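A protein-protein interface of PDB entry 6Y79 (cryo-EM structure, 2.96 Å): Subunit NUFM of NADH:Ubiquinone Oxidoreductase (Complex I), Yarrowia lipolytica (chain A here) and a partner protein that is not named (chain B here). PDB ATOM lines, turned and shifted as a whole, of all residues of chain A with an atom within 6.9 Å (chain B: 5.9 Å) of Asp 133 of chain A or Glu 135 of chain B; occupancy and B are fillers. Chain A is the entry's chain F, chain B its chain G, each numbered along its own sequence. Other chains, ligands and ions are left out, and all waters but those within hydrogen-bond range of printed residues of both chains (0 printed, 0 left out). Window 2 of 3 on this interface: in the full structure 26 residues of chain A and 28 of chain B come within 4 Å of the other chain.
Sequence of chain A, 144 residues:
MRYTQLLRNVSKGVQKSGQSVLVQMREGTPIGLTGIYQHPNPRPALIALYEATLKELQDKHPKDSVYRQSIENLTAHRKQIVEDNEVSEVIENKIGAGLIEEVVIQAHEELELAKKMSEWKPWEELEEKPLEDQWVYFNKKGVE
CG of Arg 134 of chain B touches O of Asp 133 of chain A, 3.3 Å away.
CB of Asn 136 of chain B touches OE1 of Gln 134 of chain A, at 3.7 Å.
Val 136 of chain A touches Tyr 131 of chain B (O to CE2, 3.7 Å).
NE2 of Gln 134 of chain A sits close to NH1 of Arg 134 of chain B, 3.5 Å away.
OD2 of Asp 133 of chain A lies within hydrogen-bond range of N of Glu 135 of chain B (2.8 Å).
O of Arg 137 of chain B is in hydrogen-bond range of N of Tyr 131 of chain B (2.8 Å).
OD1 of Asn 136 of chain B sits at hydrogen-bond distance from OG1 of Thr 160 of chain B (2.7 Å).
Of the 8 printed residues of chain B, 4 touch a printed residue of chain A.
Hydrophobic or aromatic side chains of chain B that line the printed part of chain A: Tyr 131.
Printed residues of chain A that touch a printed residue of chain B: Asp 133, Gln 134 and Val 136.
Among the printed residues, 5 pairs touch across the chains.
Among the printed residues, no Asp or Glu carboxylate lies within 4 Å of a Lys or Arg side-chain nitrogen of the other chain.
Asp 133 of chain A touches just these residues of chain B: Arg 134 and Glu 135.
Of chain A, only Asp 133 (2.8 Å) comes within 4 Å of Glu 135 of chain B.
Of the printed residues of chain B, Gln 134 of chain A touches Arg 134 (3.5 Å) and Asn 136 (3.7 Å).
Of the printed residues of chain A, Asn 136 of chain B touches Gln 134 (3.7 Å).
Printed residues of chain A within 4 Å of Tyr 131 of chain B: Val 136.
Printed residues of chain B within 4 Å of Val 136 of chain A: Tyr 131 (3.7 Å).
Of the printed residues of chain A, Arg 134 of chain B touches Asp 133 and Gln 134.
The nearest residue of chain A that does not touch Glu 135 of chain B is Leu 131 of chain A (4.2 Å).
The nearest printed residue of chain A that does not touch Arg 134 of chain B is Trp 135 of chain A (4.02 Å).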
ATOM      1  N   PRO A 130      17.732 -26.529 -13.551  1.00  0.00           N
ATOM      2  CA  PRO A 130      16.758 -25.648 -14.186  1.00  0.00           C
ATOM      3  C   PRO A 130      16.156 -26.318 -15.413  1.00  0.00           C
ATOM      4  O   PRO A 130      16.701 -27.268 -15.969  1.00  0.00           O
ATOM      5  CB  PRO A 130      17.600 -24.428 -14.564  1.00  0.00           C
ATOM      6  CG  PRO A 130      18.937 -24.992 -14.827  1.00  0.00           C
ATOM      7  CD  PRO A 130      19.115 -26.133 -13.867  1.00  0.00           C
ATOM      8  N   LEU A 131      15.014 -25.797 -15.832  1.00  0.00           N
ATOM      9  CA  LEU A 131      14.483 -26.124 -17.142  1.00  0.00           C
ATOM     10  C   LEU A 131      15.258 -25.342 -18.202  1.00  0.00           C
ATOM     11  O   LEU A 131      16.131 -24.533 -17.883  1.00  0.00           O
ATOM     12  CB  LEU A 131      12.986 -25.819 -17.180  1.00  0.00           C
ATOM     13  CG  LEU A 131      12.238 -26.557 -16.069  1.00  0.00           C
ATOM     14  CD1 LEU A 131      10.843 -26.009 -15.881  1.00  0.00           C
ATOM     15  CD2 LEU A 131      12.196 -28.046 -16.357  1.00  0.00           C
ATOM     16  N   GLU A 132      14.964 -25.595 -19.480  1.00  0.00           N
ATOM     17  CA  GLU A 132      15.718 -24.864 -20.498  1.00  0.00           C
ATOM     18  C   GLU A 132      14.943 -23.666 -21.037  1.00  0.00           C
ATOM     19  O   GLU A 132      15.548 -22.732 -21.582  1.00  0.00           O
ATOM     20  CB  GLU A 132      16.179 -25.824 -21.613  1.00  0.00           C
ATOM     21  CG  GLU A 132      17.221 -25.211 -22.589  1.00  0.00           C
ATOM     22  CD  GLU A 132      18.449 -24.569 -21.896  1.00  0.00           C
ATOM     23  OE1 GLU A 132      18.929 -25.062 -20.848  1.00  0.00           O
ATOM     24  OE2 GLU A 132      18.894 -23.506 -22.383  1.00  0.00           O
ATOM     25  N   ASP A 133      13.619 -23.631 -20.840  1.00  0.00           N
ATOM     26  CA  ASP A 133      12.925 -22.372 -21.080  1.00  0.00           C
ATOM     27  C   ASP A 133      13.306 -21.346 -20.025  1.00  0.00           C
ATOM     28  O   ASP A 133      13.289 -20.139 -20.295  1.00  0.00           O
ATOM     29  CB  ASP A 133      11.407 -22.568 -21.159  1.00  0.00           C
ATOM     30  CG  ASP A 133      10.749 -22.877 -19.818  1.00  0.00           C
ATOM     31  OD1 ASP A 133      11.394 -23.422 -18.900  1.00  0.00           O
ATOM     32  OD2 ASP A 133       9.564 -22.531 -19.683  1.00  0.00           O
ATOM     33  N   GLN A 134      13.674 -21.818 -18.836  1.00  0.00           N
ATOM     34  CA  GLN A 134      14.396 -21.013 -17.861  1.00  0.00           C
ATOM     35  C   GLN A 134      15.722 -20.527 -18.436  1.00  0.00           C
ATOM     36  O   GLN A 134      16.413 -21.263 -19.142  1.00  0.00           O
ATOM     37  CB  GLN A 134      14.646 -21.846 -16.601  1.00  0.00           C
ATOM     38  CG  GLN A 134      15.085 -21.074 -15.393  1.00  0.00           C
ATOM     39  CD  GLN A 134      14.030 -20.114 -14.919  1.00  0.00           C
ATOM     40  OE1 GLN A 134      12.842 -20.420 -14.949  1.00  0.00           O
ATOM     41  NE2 GLN A 134      14.456 -18.939 -14.478  1.00  0.00           N
ATOM     42  N   TRP A 135      16.052 -19.266 -18.140  1.00  0.00           N
ATOM     43  CA  TRP A 135      17.296 -18.574 -18.519  1.00  0.00           C
ATOM     44  C   TRP A 135      17.510 -18.466 -20.033  1.00  0.00           C
ATOM     45  O   TRP A 135      18.520 -18.923 -20.567  1.00  0.00           O
ATOM     46  CB  TRP A 135      18.541 -19.209 -17.886  1.00  0.00           C
ATOM     47  CG  TRP A 135      18.483 -19.566 -16.442  1.00  0.00           C
ATOM     48  CD1 TRP A 135      18.769 -20.778 -15.900  1.00  0.00           C
ATOM     49  CD2 TRP A 135      18.155 -18.707 -15.346  1.00  0.00           C
ATOM     50  NE1 TRP A 135      18.628 -20.736 -14.540  1.00  0.00           N
ATOM     51  CE2 TRP A 135      18.251 -19.474 -14.175  1.00  0.00           C
ATOM     52  CE3 TRP A 135      17.785 -17.366 -15.241  1.00  0.00           C
ATOM     53  CZ2 TRP A 135      17.983 -18.948 -12.922  1.00  0.00           C
ATOM     54  CZ3 TRP A 135      17.521 -16.848 -14.003  1.00  0.00           C
ATOM     55  CH2 TRP A 135      17.621 -17.634 -12.858  1.00  0.00           C
ATOM     56  N   VAL A 136      16.569 -17.821 -20.721  1.00  0.00           N
ATOM     57  CA  VAL A 136      16.835 -17.216 -22.022  1.00  0.00           C
ATOM     58  C   VAL A 136      16.391 -15.764 -21.957  1.00  0.00           C
ATOM     59  O   VAL A 136      15.365 -15.448 -21.342  1.00  0.00           O
ATOM     60  CB  VAL A 136      16.171 -17.963 -23.205  1.00  0.00           C
ATOM     61  CG1 VAL A 136      16.811 -19.333 -23.406  1.00  0.00           C
ATOM     62  CG2 VAL A 136      14.650 -18.092 -23.051  1.00  0.00           C
ATOM     63  N   TYR B 131       8.744 -12.979 -17.021  1.00  0.00           N
ATOM     64  CA  TYR B 131       8.755 -13.418 -18.403  1.00  0.00           C
ATOM     65  C   TYR B 131       7.588 -14.373 -18.530  1.00  0.00           C
ATOM     66  O   TYR B 131       7.669 -15.495 -18.016  1.00  0.00           O
ATOM     67  CB  TYR B 131      10.063 -14.116 -18.772  1.00  0.00           C
ATOM     68  CG  TYR B 131      11.302 -13.242 -18.834  1.00  0.00           C
ATOM     69  CD1 TYR B 131      11.243 -11.892 -18.593  1.00  0.00           C
ATOM     70  CD2 TYR B 131      12.525 -13.773 -19.188  1.00  0.00           C
ATOM     71  CE1 TYR B 131      12.352 -11.115 -18.650  1.00  0.00           C
ATOM     72  CE2 TYR B 131      13.646 -12.981 -19.258  1.00  0.00           C
ATOM     73  CZ  TYR B 131      13.541 -11.646 -18.984  1.00  0.00           C
ATOM     74  OH  TYR B 131      14.611 -10.797 -19.036  1.00  0.00           O
ATOM     75  N   PRO B 132       6.470 -13.982 -19.147  1.00  0.00           N
ATOM     76  CA  PRO B 132       5.304 -14.877 -19.182  1.00  0.00           C
ATOM     77  C   PRO B 132       5.477 -16.091 -20.083  1.00  0.00           C
ATOM     78  O   PRO B 132       4.653 -17.007 -20.009  1.00  0.00           O
ATOM     79  CB  PRO B 132       4.182 -13.962 -19.683  1.00  0.00           C
ATOM     80  CG  PRO B 132       4.868 -12.885 -20.413  1.00  0.00           C
ATOM     81  CD  PRO B 132       6.162 -12.660 -19.713  1.00  0.00           C
ATOM     82  N   SER B 133       6.520 -16.139 -20.908  1.00  0.00           N
ATOM     83  CA  SER B 133       6.746 -17.280 -21.780  1.00  0.00           C
ATOM     84  C   SER B 133       7.463 -18.427 -21.085  1.00  0.00           C
ATOM     85  O   SER B 133       7.581 -19.506 -21.671  1.00  0.00           O
ATOM     86  CB  SER B 133       7.538 -16.846 -23.008  1.00  0.00           C
ATOM     87  OG  SER B 133       8.629 -16.030 -22.636  1.00  0.00           O
ATOM     88  N   ARG B 134       7.943 -18.228 -19.865  1.00  0.00           N
ATOM     89  CA  ARG B 134       8.596 -19.285 -19.112  1.00  0.00           C
ATOM     90  C   ARG B 134       7.597 -20.010 -18.217  1.00  0.00           C
ATOM     91  O   ARG B 134       6.532 -19.476 -17.894  1.00  0.00           O
ATOM     92  CB  ARG B 134       9.731 -18.710 -18.272  1.00  0.00           C
ATOM     93  CG  ARG B 134      10.899 -18.271 -19.097  1.00  0.00           C
ATOM     94  CD  ARG B 134      12.051 -17.833 -18.240  1.00  0.00           C
ATOM     95  NE  ARG B 134      11.663 -16.730 -17.383  1.00  0.00           N
ATOM     96  CZ  ARG B 134      12.503 -16.028 -16.635  1.00  0.00           C
ATOM     97  NH1 ARG B 134      13.801 -16.298 -16.641  1.00  0.00           N
ATOM     98  NH2 ARG B 134      12.038 -15.033 -15.895  1.00  0.00           N
ATOM     99  N   GLU B 135       7.944 -21.249 -17.841  1.00  0.00           N
ATOM    100  CA  GLU B 135       7.137 -21.988 -16.871  1.00  0.00           C
ATOM    101  C   GLU B 135       7.138 -21.288 -15.523  1.00  0.00           C
ATOM    102  O   GLU B 135       6.078 -21.020 -14.948  1.00  0.00           O
ATOM    103  CB  GLU B 135       7.660 -23.416 -16.692  1.00  0.00           C
ATOM    104  CG  GLU B 135       7.569 -24.339 -17.895  1.00  0.00           C
ATOM    105  CD  GLU B 135       6.154 -24.694 -18.289  1.00  0.00           C
ATOM    106  OE1 GLU B 135       5.281 -24.744 -17.403  1.00  0.00           O
ATOM    107  OE2 GLU B 135       5.919 -24.939 -19.489  1.00  0.00           O
ATOM    108  N   ASN B 136       8.322 -20.989 -15.008  1.00  0.00           N
ATOM    109  CA  ASN B 136       8.480 -20.209 -13.789  1.00  0.00           C
ATOM    110  C   ASN B 136       8.518 -18.749 -14.206  1.00  0.00           C
ATOM    111  O   ASN B 136       9.505 -18.277 -14.772  1.00  0.00           O
ATOM    112  CB  ASN B 136       9.734 -20.639 -13.045  1.00  0.00           C
ATOM    113  CG  ASN B 136       9.625 -22.046 -12.519  1.00  0.00           C
ATOM    114  OD1 ASN B 136       9.022 -22.286 -11.480  1.00  0.00           O
ATOM    115  ND2 ASN B 136      10.192 -22.992 -13.249  1.00  0.00           N
ATOM    116  N   ARG B 137       7.430 -18.039 -13.910  1.00  0.00           N
ATOM    117  CA  ARG B 137       7.114 -16.782 -14.580  1.00  0.00           C
ATOM    118  C   ARG B 137       8.050 -15.666 -14.154  1.00  0.00           C
ATOM    119  O   ARG B 137       8.586 -14.936 -14.992  1.00  0.00           O
ATOM    120  CB  ARG B 137       5.667 -16.413 -14.276  1.00  0.00           C
ATOM    121  CG  ARG B 137       5.206 -15.122 -14.860  1.00  0.00           C
ATOM    122  CD  ARG B 137       3.760 -14.899 -14.524  1.00  0.00           C
ATOM    123  NE  ARG B 137       3.220 -13.771 -15.264  1.00  0.00           N
ATOM    124  CZ  ARG B 137       1.970 -13.348 -15.165  1.00  0.00           C
ATOM    125  NH1 ARG B 137       1.128 -13.961 -14.351  1.00  0.00           N
ATOM    126  NH2 ARG B 137       1.566 -12.310 -15.878  1.00  0.00           N
ATOM    127  N   THR B 160       7.400 -19.187  -9.575  1.00  0.00           N
ATOM    128  CA  THR B 160       6.086 -19.115 -10.179  1.00  0.00           C
ATOM    129  C   THR B 160       5.199 -18.233  -9.301  1.00  0.00           C
ATOM    130  O   THR B 160       5.543 -17.911  -8.164  1.00  0.00           O
ATOM    131  CB  THR B 160       5.514 -20.529 -10.359  1.00  0.00           C
ATOM    132  OG1 THR B 160       6.569 -21.400 -10.776  1.00  0.00           O
ATOM    133  CG2 THR B 160       4.430 -20.598 -11.445  1.00  0.00           C
